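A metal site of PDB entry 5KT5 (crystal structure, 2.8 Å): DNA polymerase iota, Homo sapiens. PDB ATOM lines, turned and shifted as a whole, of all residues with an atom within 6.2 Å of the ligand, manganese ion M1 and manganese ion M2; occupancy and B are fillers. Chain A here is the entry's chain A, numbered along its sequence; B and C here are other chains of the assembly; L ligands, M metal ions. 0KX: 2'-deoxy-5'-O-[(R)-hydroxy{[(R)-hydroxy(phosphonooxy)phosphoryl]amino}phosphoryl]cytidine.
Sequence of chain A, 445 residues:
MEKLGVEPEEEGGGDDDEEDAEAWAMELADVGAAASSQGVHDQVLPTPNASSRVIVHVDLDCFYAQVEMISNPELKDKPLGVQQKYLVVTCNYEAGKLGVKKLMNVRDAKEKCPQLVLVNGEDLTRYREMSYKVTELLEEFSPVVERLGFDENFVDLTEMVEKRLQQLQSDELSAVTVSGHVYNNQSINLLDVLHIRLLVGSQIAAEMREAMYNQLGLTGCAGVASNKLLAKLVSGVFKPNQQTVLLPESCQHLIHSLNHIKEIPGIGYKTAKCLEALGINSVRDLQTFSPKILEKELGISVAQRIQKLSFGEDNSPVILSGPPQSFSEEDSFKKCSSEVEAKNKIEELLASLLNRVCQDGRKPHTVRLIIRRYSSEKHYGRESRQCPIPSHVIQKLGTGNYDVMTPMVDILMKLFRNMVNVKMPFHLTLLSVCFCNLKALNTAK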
ATOM      1  N   ASP A  59      12.256   5.526  -8.667  1.00  0.00           N
ATOM      2  CA  ASP A  59      13.575   4.926  -8.794  1.00  0.00           C
ATOM      3  C   ASP A  59      13.653   3.736  -7.836  1.00  0.00           C
ATOM      4  O   ASP A  59      13.384   3.890  -6.642  1.00  0.00           O
ATOM      5  CB  ASP A  59      14.669   5.949  -8.464  1.00  0.00           C
ATOM      6  CG  ASP A  59      16.084   5.394  -8.614  1.00  0.00           C
ATOM      7  OD1 ASP A  59      16.900   6.036  -9.301  1.00  0.00           O
ATOM      8  OD2 ASP A  59      16.398   4.337  -8.037  1.00  0.00           O
ATOM      9  N   LEU A  60      14.034   2.581  -8.342  1.00  0.00           N
ATOM     10  CA  LEU A  60      14.026   1.361  -7.536  1.00  0.00           C
ATOM     11  C   LEU A  60      15.247   1.313  -6.621  1.00  0.00           C
ATOM     12  O   LEU A  60      16.345   1.694  -7.005  1.00  0.00           O
ATOM     13  CB  LEU A  60      14.002   0.134  -8.435  1.00  0.00           C
ATOM     14  CG  LEU A  60      12.771   0.093  -9.344  1.00  0.00           C
ATOM     15  CD1 LEU A  60      12.699  -1.201 -10.128  1.00  0.00           C
ATOM     16  CD2 LEU A  60      11.529   0.273  -8.498  1.00  0.00           C
ATOM     17  N   ASP A  61      15.019   0.835  -5.395  1.00  0.00           N
ATOM     18  CA  ASP A  61      16.108   0.645  -4.441  1.00  0.00           C
ATOM     19  C   ASP A  61      17.019  -0.488  -4.890  1.00  0.00           C
ATOM     20  O   ASP A  61      16.543  -1.594  -5.156  1.00  0.00           O
ATOM     21  CB  ASP A  61      15.536   0.334  -3.060  1.00  0.00           C
ATOM     22  CG  ASP A  61      14.570   1.407  -2.554  1.00  0.00           C
ATOM     23  OD1 ASP A  61      14.922   2.609  -2.589  1.00  0.00           O
ATOM     24  OD2 ASP A  61      13.461   1.040  -2.122  1.00  0.00           O
ATOM     25  N   CYS A  62      18.329  -0.198  -4.946  1.00  0.00           N
ATOM     26  CA  CYS A  62      19.380  -1.126  -5.359  1.00  0.00           C
ATOM     27  C   CYS A  62      18.869  -2.199  -6.307  1.00  0.00           C
ATOM     28  O   CYS A  62      18.779  -3.375  -5.946  1.00  0.00           O
ATOM     29  CB  CYS A  62      20.041  -1.778  -4.132  1.00  0.00           C
ATOM     30  SG  CYS A  62      18.885  -2.451  -2.907  1.00  0.00           S
ATOM     31  N   PHE A  63      18.531  -1.789  -7.531  1.00  0.00           N
ATOM     32  CA  PHE A  63      17.637  -2.570  -8.373  1.00  0.00           C
ATOM     33  C   PHE A  63      18.136  -4.006  -8.572  1.00  0.00           C
ATOM     34  O   PHE A  63      17.500  -4.978  -8.149  1.00  0.00           O
ATOM     35  CB  PHE A  63      17.442  -1.846  -9.702  1.00  0.00           C
ATOM     36  CG  PHE A  63      16.560  -2.593 -10.675  1.00  0.00           C
ATOM     37  CD1 PHE A  63      15.413  -3.249 -10.258  1.00  0.00           C
ATOM     38  CD2 PHE A  63      16.893  -2.631 -12.028  1.00  0.00           C
ATOM     39  CE1 PHE A  63      14.617  -3.930 -11.158  1.00  0.00           C
ATOM     40  CE2 PHE A  63      16.105  -3.312 -12.924  1.00  0.00           C
ATOM     41  CZ  PHE A  63      14.963  -3.961 -12.491  1.00  0.00           C
ATOM     42  N   TYR A  64      19.295  -4.144  -9.229  1.00  0.00           N
ATOM     43  CA  TYR A  64      19.857  -5.465  -9.483  1.00  0.00           C
ATOM     44  C   TYR A  64      19.948  -6.298  -8.206  1.00  0.00           C
ATOM     45  O   TYR A  64      19.554  -7.473  -8.177  1.00  0.00           O
ATOM     46  CB  TYR A  64      21.248  -5.335 -10.121  1.00  0.00           C
ATOM     47  CG  TYR A  64      21.271  -4.743 -11.515  1.00  0.00           C
ATOM     48  CD1 TYR A  64      20.105  -4.326 -12.157  1.00  0.00           C
ATOM     49  CD2 TYR A  64      22.463  -4.626 -12.218  1.00  0.00           C
ATOM     50  CE1 TYR A  64      20.134  -3.792 -13.433  1.00  0.00           C
ATOM     51  CE2 TYR A  64      22.500  -4.093 -13.490  1.00  0.00           C
ATOM     52  CZ  TYR A  64      21.340  -3.675 -14.096  1.00  0.00           C
ATOM     53  OH  TYR A  64      21.389  -3.151 -15.367  1.00  0.00           O
ATOM     54  N   ALA A  65      20.464  -5.691  -7.129  1.00  0.00           N
ATOM     55  CA  ALA A  65      20.595  -6.423  -5.877  1.00  0.00           C
ATOM     56  C   ALA A  65      19.230  -6.840  -5.329  1.00  0.00           C
ATOM     57  O   ALA A  65      19.092  -7.904  -4.712  1.00  0.00           O
ATOM     58  CB  ALA A  65      21.338  -5.582  -4.843  1.00  0.00           C
ATOM     59  N   GLN A  84      29.843  -6.926 -12.260  1.00  0.00           N
ATOM     60  CA  GLN A  84      30.017  -7.077 -13.712  1.00  0.00           C
ATOM     61  C   GLN A  84      31.485  -6.808 -14.010  1.00  0.00           C
ATOM     62  O   GLN A  84      31.948  -5.676 -13.865  1.00  0.00           O
ATOM     63  CB  GLN A  84      29.118  -6.121 -14.492  1.00  0.00           C
ATOM     64  CG  GLN A  84      27.631  -6.395 -14.354  1.00  0.00           C
ATOM     65  CD  GLN A  84      26.784  -5.319 -14.984  1.00  0.00           C
ATOM     66  OE1 GLN A  84      27.177  -4.146 -15.037  1.00  0.00           O
ATOM     67  NE2 GLN A  84      25.613  -5.698 -15.471  1.00  0.00           N
ATOM     68  N   VAL A  89      28.492  -3.133  -9.397  1.00  0.00           N
ATOM     69  CA  VAL A  89      27.617  -2.156 -10.031  1.00  0.00           C
ATOM     70  C   VAL A  89      26.560  -1.630  -9.064  1.00  0.00           C
ATOM     71  O   VAL A  89      26.049  -0.514  -9.239  1.00  0.00           O
ATOM     72  CB  VAL A  89      26.988  -2.752 -11.301  1.00  0.00           C
ATOM     73  CG1 VAL A  89      25.648  -3.417 -10.992  1.00  0.00           C
ATOM     74  CG2 VAL A  89      26.824  -1.685 -12.354  1.00  0.00           C
ATOM     75  N   THR A  90      26.198  -2.425  -8.053  1.00  0.00           N
ATOM     76  CA  THR A  90      25.300  -1.976  -6.993  1.00  0.00           C
ATOM     77  C   THR A  90      25.356  -2.989  -5.871  1.00  0.00           C
ATOM     78  O   THR A  90      25.950  -4.070  -5.993  1.00  0.00           O
ATOM     79  CB  THR A  90      23.849  -1.807  -7.483  1.00  0.00           C
ATOM     80  OG1 THR A  90      23.068  -1.230  -6.427  1.00  0.00           O
ATOM     81  CG2 THR A  90      23.259  -3.151  -7.868  1.00  0.00           C
ATOM     82  N   CYS A  91      24.731  -2.627  -4.754  1.00  0.00           N
ATOM     83  CA  CYS A  91      24.800  -3.450  -3.552  1.00  0.00           C
ATOM     84  C   CYS A  91      23.566  -3.194  -2.707  1.00  0.00           C
ATOM     85  O   CYS A  91      22.936  -2.134  -2.803  1.00  0.00           O
ATOM     86  CB  CYS A  91      26.082  -3.171  -2.759  1.00  0.00           C
ATOM     87  SG  CYS A  91      26.202  -1.517  -2.043  1.00  0.00           S
ATOM     88  N   LYS A 102      28.128   2.093  -4.853  1.00  0.00           N
ATOM     89  CA  LYS A 102      27.808   1.723  -6.228  1.00  0.00           C
ATOM     90  C   LYS A 102      28.955   2.084  -7.153  1.00  0.00           C
ATOM     91  O   LYS A 102      29.597   3.132  -7.013  1.00  0.00           O
ATOM     92  CB  LYS A 102      26.519   2.424  -6.660  1.00  0.00           C
ATOM     93  CG  LYS A 102      25.297   2.029  -5.837  1.00  0.00           C
ATOM     94  CD  LYS A 102      24.077   2.867  -6.163  1.00  0.00           C
ATOM     95  CE  LYS A 102      24.165   4.262  -5.551  1.00  0.00           C
ATOM     96  NZ  LYS A 102      22.873   5.016  -5.652  1.00  0.00           N
ATOM     97  N   LEU A 103      29.219   1.196  -8.120  1.00  0.00           N
ATOM     98  CA  LEU A 103      30.279   1.381  -9.106  1.00  0.00           C
ATOM     99  C   LEU A 103      31.669   1.419  -8.466  1.00  0.00           C
ATOM    100  O   LEU A 103      32.583   2.088  -8.952  1.00  0.00           O
ATOM    101  CB  LEU A 103      30.041   2.644  -9.950  1.00  0.00           C
ATOM    102  CG  LEU A 103      28.649   2.713 -10.594  1.00  0.00           C
ATOM    103  CD1 LEU A 103      28.399   4.075 -11.220  1.00  0.00           C
ATOM    104  CD2 LEU A 103      28.489   1.621 -11.623  1.00  0.00           C
ATOM    105  N   LEU A 124      21.550  -9.218 -18.103  1.00  0.00           N
ATOM    106  CA  LEU A 124      20.504  -8.293 -17.676  1.00  0.00           C
ATOM    107  C   LEU A 124      19.092  -8.809 -17.971  1.00  0.00           C
ATOM    108  O   LEU A 124      18.148  -8.011 -17.921  1.00  0.00           O
ATOM    109  CB  LEU A 124      20.696  -6.940 -18.364  1.00  0.00           C
ATOM    110  CG  LEU A 124      22.099  -6.329 -18.438  1.00  0.00           C
ATOM    111  CD1 LEU A 124      22.018  -4.941 -19.053  1.00  0.00           C
ATOM    112  CD2 LEU A 124      22.762  -6.280 -17.071  1.00  0.00           C
ATOM    113  N   LEU A 148      13.444   5.978 -17.817  1.00  0.00           N
ATOM    114  CA  LEU A 148      14.837   6.385 -17.722  1.00  0.00           C
ATOM    115  C   LEU A 148      15.612   5.232 -17.095  1.00  0.00           C
ATOM    116  O   LEU A 148      15.329   4.845 -15.948  1.00  0.00           O
ATOM    117  CB  LEU A 148      15.016   7.676 -16.907  1.00  0.00           C
ATOM    118  CG  LEU A 148      16.384   8.338 -17.056  1.00  0.00           C
ATOM    119  CD1 LEU A 148      16.714   8.539 -18.523  1.00  0.00           C
ATOM    120  CD2 LEU A 148      16.449   9.664 -16.309  1.00  0.00           C
ATOM    121  N   PHE A 150      16.866   1.303 -16.582  1.00  0.00           N
ATOM    122  CA  PHE A 150      16.032   0.147 -16.291  1.00  0.00           C
ATOM    123  C   PHE A 150      15.158   0.353 -15.062  1.00  0.00           C
ATOM    124  O   PHE A 150      14.177  -0.384 -14.897  1.00  0.00           O
ATOM    125  CB  PHE A 150      16.903  -1.088 -16.082  1.00  0.00           C
ATOM    126  CG  PHE A 150      17.350  -1.746 -17.367  1.00  0.00           C
ATOM    127  CD1 PHE A 150      17.965  -2.986 -17.348  1.00  0.00           C
ATOM    128  CD2 PHE A 150      17.156  -1.131 -18.588  1.00  0.00           C
ATOM    129  CE1 PHE A 150      18.372  -3.603 -18.518  1.00  0.00           C
ATOM    130  CE2 PHE A 150      17.554  -1.726 -19.765  1.00  0.00           C
ATOM    131  CZ  PHE A 150      18.164  -2.960 -19.734  1.00  0.00           C
ATOM    132  N   ASP A 151      15.462   1.324 -14.206  1.00  0.00           N
ATOM    133  CA  ASP A 151      14.831   1.388 -12.898  1.00  0.00           C
ATOM    134  C   ASP A 151      14.168   2.726 -12.587  1.00  0.00           C
ATOM    135  O   ASP A 151      13.784   2.949 -11.437  1.00  0.00           O
ATOM    136  CB  ASP A 151      15.844   1.044 -11.806  1.00  0.00           C
ATOM    137  CG  ASP A 151      16.600   2.256 -11.289  1.00  0.00           C
ATOM    138  OD1 ASP A 151      17.033   3.099 -12.113  1.00  0.00           O
ATOM    139  OD2 ASP A 151      16.747   2.383 -10.048  1.00  0.00           O
ATOM    140  N   GLU A 152      14.019   3.631 -13.560  1.00  0.00           N
ATOM    141  CA  GLU A 152      13.371   4.908 -13.278  1.00  0.00           C
ATOM    142  C   GLU A 152      12.234   5.160 -14.251  1.00  0.00           C
ATOM    143  O   GLU A 152      12.319   4.821 -15.433  1.00  0.00           O
ATOM    144  CB  GLU A 152      14.385   6.053 -13.303  1.00  0.00           C
ATOM    145  CG  GLU A 152      15.374   5.972 -12.151  1.00  0.00           C
ATOM    146  CD  GLU A 152      16.471   6.999 -12.258  1.00  0.00           C
ATOM    147  OE1 GLU A 152      16.211   8.093 -12.786  1.00  0.00           O
ATOM    148  OE2 GLU A 152      17.596   6.712 -11.811  1.00  0.00           O
ATOM    149  N   LYS A 239      15.874   7.987   1.340  1.00  0.00           N
ATOM    150  CA  LYS A 239      16.137   6.656   0.819  1.00  0.00           C
ATOM    151  C   LYS A 239      16.493   5.695   1.948  1.00  0.00           C
ATOM    152  O   LYS A 239      17.082   6.116   2.947  1.00  0.00           O
ATOM    153  CB  LYS A 239      17.271   6.702  -0.224  1.00  0.00           C
ATOM    154  CG  LYS A 239      16.867   7.297  -1.564  1.00  0.00           C
ATOM    155  CD  LYS A 239      18.076   7.629  -2.428  1.00  0.00           C
ATOM    156  CE  LYS A 239      19.078   6.479  -2.478  1.00  0.00           C
ATOM    157  NZ  LYS A 239      20.245   6.793  -3.345  1.00  0.00           N
ATOM    158  N   PRO A 240      16.136   4.412   1.799  1.00  0.00           N
ATOM    159  CA  PRO A 240      15.377   3.853   0.675  1.00  0.00           C
ATOM    160  C   PRO A 240      13.894   3.710   0.970  1.00  0.00           C
ATOM    161  O   PRO A 240      13.474   3.953   2.102  1.00  0.00           O
ATOM    162  CB  PRO A 240      16.016   2.477   0.500  1.00  0.00           C
ATOM    163  CG  PRO A 240      16.319   2.067   1.905  1.00  0.00           C
ATOM    164  CD  PRO A 240      16.672   3.341   2.671  1.00  0.00           C
ATOM    165  P    DC B   7      21.151   9.872 -14.191  1.00  0.00           P
ATOM    166  OP1  DC B   7      20.400  10.513 -13.085  1.00  0.00           O
ATOM    167  OP2  DC B   7      22.596  10.148 -14.357  1.00  0.00           O
ATOM    168  O5'  DC B   7      20.944   8.295 -14.105  1.00  0.00           O
ATOM    169  C5'  DC B   7      19.619   7.761 -14.094  1.00  0.00           C
ATOM    170  C4'  DC B   7      19.631   6.251 -14.295  1.00  0.00           C
ATOM    171  O4'  DC B   7      20.139   5.941 -15.601  1.00  0.00           O
ATOM    172  C3'  DC B   7      20.530   5.467 -13.355  1.00  0.00           C
ATOM    173  O3'  DC B   7      19.878   5.268 -12.102  1.00  0.00           O
ATOM    174  C2'  DC B   7      20.688   4.163 -14.116  1.00  0.00           C
ATOM    175  C1'  DC B   7      20.711   4.639 -15.578  1.00  0.00           C
ATOM    176  N1   DC B   7      22.076   4.710 -16.147  1.00  0.00           N
ATOM    177  C2   DC B   7      22.694   3.539 -16.572  1.00  0.00           C
ATOM    178  O2   DC B   7      22.071   2.483 -16.476  1.00  0.00           O
ATOM    179  N3   DC B   7      23.957   3.606 -17.081  1.00  0.00           N
ATOM    180  C4   DC B   7      24.576   4.782 -17.154  1.00  0.00           C
ATOM    181  N4   DC B   7      25.807   4.800 -17.661  1.00  0.00           N
ATOM    182  C5   DC B   7      23.964   5.995 -16.721  1.00  0.00           C
ATOM    183  C6   DC B   7      22.717   5.913 -16.223  1.00  0.00           C
ATOM    184  P    DG C   3      35.454  -2.909 -17.136  1.00  0.00           P
ATOM    185  OP1  DG C   3      36.579  -3.861 -17.136  1.00  0.00           O
ATOM    186  OP2  DG C   3      35.338  -1.909 -18.218  1.00  0.00           O
ATOM    187  O5'  DG C   3      34.069  -3.702 -17.114  1.00  0.00           O
ATOM    188  C5'  DG C   3      32.908  -3.069 -16.574  1.00  0.00           C
ATOM    189  C4'  DG C   3      31.702  -3.977 -16.628  1.00  0.00           C
ATOM    190  O4'  DG C   3      30.585  -3.334 -15.962  1.00  0.00           O
ATOM    191  C3'  DG C   3      31.192  -4.310 -18.021  1.00  0.00           C
ATOM    192  O3'  DG C   3      30.491  -5.544 -17.982  1.00  0.00           O
ATOM    193  C2'  DG C   3      30.253  -3.141 -18.295  1.00  0.00           C
ATOM    194  C1'  DG C   3      29.618  -2.942 -16.912  1.00  0.00           C
ATOM    195  N9   DG C   3      29.202  -1.564 -16.621  1.00  0.00           N
ATOM    196  C8   DG C   3      28.021  -1.182 -16.038  1.00  0.00           C
ATOM    197  N7   DG C   3      27.922   0.110 -15.869  1.00  0.00           N
ATOM    198  C5   DG C   3      29.117   0.616 -16.359  1.00  0.00           C
ATOM    199  C6   DG C   3      29.580   1.947 -16.436  1.00  0.00           C
ATOM    200  O6   DG C   3      29.006   2.988 -16.079  1.00  0.00           O
ATOM    201  N1   DG C   3      30.856   2.025 -17.004  1.00  0.00           N
ATOM    202  C2   DG C   3      31.582   0.937 -17.432  1.00  0.00           C
ATOM    203  N2   DG C   3      32.787   1.211 -17.953  1.00  0.00           N
ATOM    204  N3   DG C   3      31.164  -0.319 -17.365  1.00  0.00           N
ATOM    205  C4   DG C   3      29.929  -0.404 -16.817  1.00  0.00           C
ATOM    206  P    DG C   4      30.251  -6.410 -19.323  1.00  0.00           P
ATOM    207  OP1  DG C   4      30.461  -7.837 -18.981  1.00  0.00           O
ATOM    208  OP2  DG C   4      31.026  -5.794 -20.417  1.00  0.00           O
ATOM    209  O5'  DG C   4      28.700  -6.188 -19.638  1.00  0.00           O
ATOM    210  C5'  DG C   4      27.732  -6.447 -18.633  1.00  0.00           C
ATOM    211  C4'  DG C   4      26.418  -5.768 -18.980  1.00  0.00           C
ATOM    212  O4'  DG C   4      26.470  -4.378 -18.536  1.00  0.00           O
ATOM    213  C3'  DG C   4      26.101  -5.715 -20.474  1.00  0.00           C
ATOM    214  O3'  DG C   4      24.711  -5.986 -20.687  1.00  0.00           O
ATOM    215  C2'  DG C   4      26.453  -4.280 -20.833  1.00  0.00           C
ATOM    216  C1'  DG C   4      26.005  -3.571 -19.574  1.00  0.00           C
ATOM    217  N9   DG C   4      26.518  -2.206 -19.467  1.00  0.00           N
ATOM    218  C8   DG C   4      27.729  -1.731 -19.917  1.00  0.00           C
ATOM    219  N7   DG C   4      27.893  -0.451 -19.700  1.00  0.00           N
ATOM    220  C5   DG C   4      26.723  -0.062 -19.064  1.00  0.00           C
ATOM    221  C6   DG C   4      26.320   1.206 -18.592  1.00  0.00           C
ATOM    222  O6   DG C   4      26.947   2.275 -18.623  1.00  0.00           O
ATOM    223  N1   DG C   4      25.051   1.161 -18.019  1.00  0.00           N
ATOM    224  C2   DG C   4      24.268   0.034 -17.926  1.00  0.00           C
ATOM    225  N2   DG C   4      23.069   0.172 -17.355  1.00  0.00           N
ATOM    226  N3   DG C   4      24.636  -1.163 -18.373  1.00  0.00           N
ATOM    227  C4   DG C   4      25.866  -1.129 -18.932  1.00  0.00           C
HETATM  228  PG  0KX L   1      19.558   3.137  -5.433  1.00  0.00           P
HETATM  229  O1G 0KX L   1      18.588   3.521  -6.526  1.00  0.00           O
HETATM  230  O2G 0KX L   1      20.664   4.150  -5.230  1.00  0.00           O
HETATM  231  O3G 0KX L   1      18.899   2.666  -4.164  1.00  0.00           O
HETATM  232  PB  0KX L   1      20.458   1.509  -7.559  1.00  0.00           P
HETATM  233  O1B 0KX L   1      21.243   0.217  -7.651  1.00  0.00           O
HETATM  234  O2B 0KX L   1      19.071   1.511  -8.158  1.00  0.00           O
HETATM  235  O3B 0KX L   1      20.316   1.831  -5.992  1.00  0.00           O
HETATM  236  PA  0KX L   1      20.819   3.330  -9.871  1.00  0.00           P
HETATM  237  O1A 0KX L   1      21.744   4.435 -10.317  1.00  0.00           O
HETATM  238  O2A 0KX L   1      19.347   3.658  -9.742  1.00  0.00           O
HETATM  239  N3A 0KX L   1      21.433   2.776  -8.313  1.00  0.00           N
HETATM  240  O5' 0KX L   1      20.925   2.171 -10.977  1.00  0.00           O
HETATM  241  C5' 0KX L   1      19.876   1.217 -11.168  1.00  0.00           C
HETATM  242  C4' 0KX L   1      20.534  -0.059 -11.675  1.00  0.00           C
HETATM  243  O4' 0KX L   1      21.147   0.179 -12.940  1.00  0.00           O
HETATM  244  C3' 0KX L   1      21.643  -0.505 -10.745  1.00  0.00           C
HETATM  245  O3' 0KX L   1      21.201  -1.526  -9.833  1.00  0.00           O
HETATM  246  C2' 0KX L   1      22.731  -1.042 -11.657  1.00  0.00           C
HETATM  247  C1' 0KX L   1      22.421  -0.471 -13.036  1.00  0.00           C
HETATM  248  N1  0KX L   1      23.467   0.493 -13.373  1.00  0.00           N
HETATM  249  C2  0KX L   1      24.578   0.129 -14.151  1.00  0.00           C
HETATM  250  N3  0KX L   1      25.536   1.037 -14.430  1.00  0.00           N
HETATM  251  C4  0KX L   1      25.433   2.309 -13.971  1.00  0.00           C
HETATM  252  C5  0KX L   1      24.339   2.680 -13.207  1.00  0.00           C
HETATM  253  C6  0KX L   1      23.354   1.742 -12.915  1.00  0.00           C
HETATM  254  O2  0KX L   1      24.687  -1.045 -14.581  1.00  0.00           O
HETATM  255  N4  0KX L   1      26.395   3.221 -14.259  1.00  0.00           N
HETATM  256 MN    MN M   1      17.707   2.841  -8.268  1.00  0.00          MN
HETATM  257 MN    MN M   2      18.235   4.769 -10.722  1.00  0.00          MN
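N2 of DG 4 of chain C sits close to an oxygen (O2) of the ligand (3.4 Å). Asp 61 touches the ligand. Val 89 touches the ligand. Leu 103 touches the ligand. Hydrophobic or aromatic side chains within 4 Å of the ligand: Phe 63, Tyr 64, Val 89 and Leu 103. Of the 23 residues printed, 15 come within 4 Å of the ligand.
The side-chain amino group (NZ) of Lys 102 is in salt-bridge range of an oxygen (O2G) of the ligand. OG1 of Thr 90 is in hydrogen-bond range of O1B of the ligand (2.6 Å). O6 of DG 3 of chain C is in hydrogen-bond range of N4 of the ligand (3.2 Å). O3G of the ligand sits at hydrogen-bond distance from N of Cys 62. An oxygen (O2G) of the ligand is in salt-bridge range of the side-chain amino group (NZ) of Lys 239. The backbone NH of Tyr 64 sits at hydrogen-bond distance from an oxygen (O3') of the ligand (3.3 Å). An oxygen (O1B) of the ligand lies within hydrogen-bond range of the backbone NH (N) of Phe 63 (3.4 Å).
Manganese ion M2 is bound by O2A of the ligand (1.9 Å), O3' of DC 7 of chain B (2.2 Å), OE2 of Glu 152 (2.3 Å), OD1 of Asp 59 (2.3 Å) and OD1 of Asp 151 (2.5 Å). Manganese ion M2 has five donor atoms within binding distance. Slightly farther from manganese ion M2 lies the side-chain carboxylate (OD2) of Asp 151 (2.9 Å).
N2 of DG 4 of chain C lies close to O2 of DC 7 of chain B, 2.7 Å away. The side-chain amide nitrogen of Gln 84 lies within hydrogen-bond range of O4' of DG 4 of chain C, 3.4 Å away.
Three residues have an atom within 4 Å of manganese ion M1: Asp 59, Leu 60 and Asp 151. The nearest printed residue that does not touch manganese ion M1 is Asp 61 (4.4 Å).
O2B of the ligand is bound to manganese ion M1 (1.9 Å). OD2 of Asp 59 binds manganese ion M1 (2.0 Å). An oxygen (O1G) of the ligand is bound to manganese ion M1 (2.1 Å). The side-chain carboxylate (OD2) of Asp 151 is bound to manganese ion M1, 2.1 Å away. The backbone carbonyl oxygen (O) of Leu 60 is bound to manganese ion M1 (2.2 Å). An oxygen (O2A) of the ligand is bound to manganese ion M1, at 2.4 Å.
Four residues have an atom within 4 Å of manganese ion M2: Asp 59, Asp 151, Glu 152 and DC 7 of chain B.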
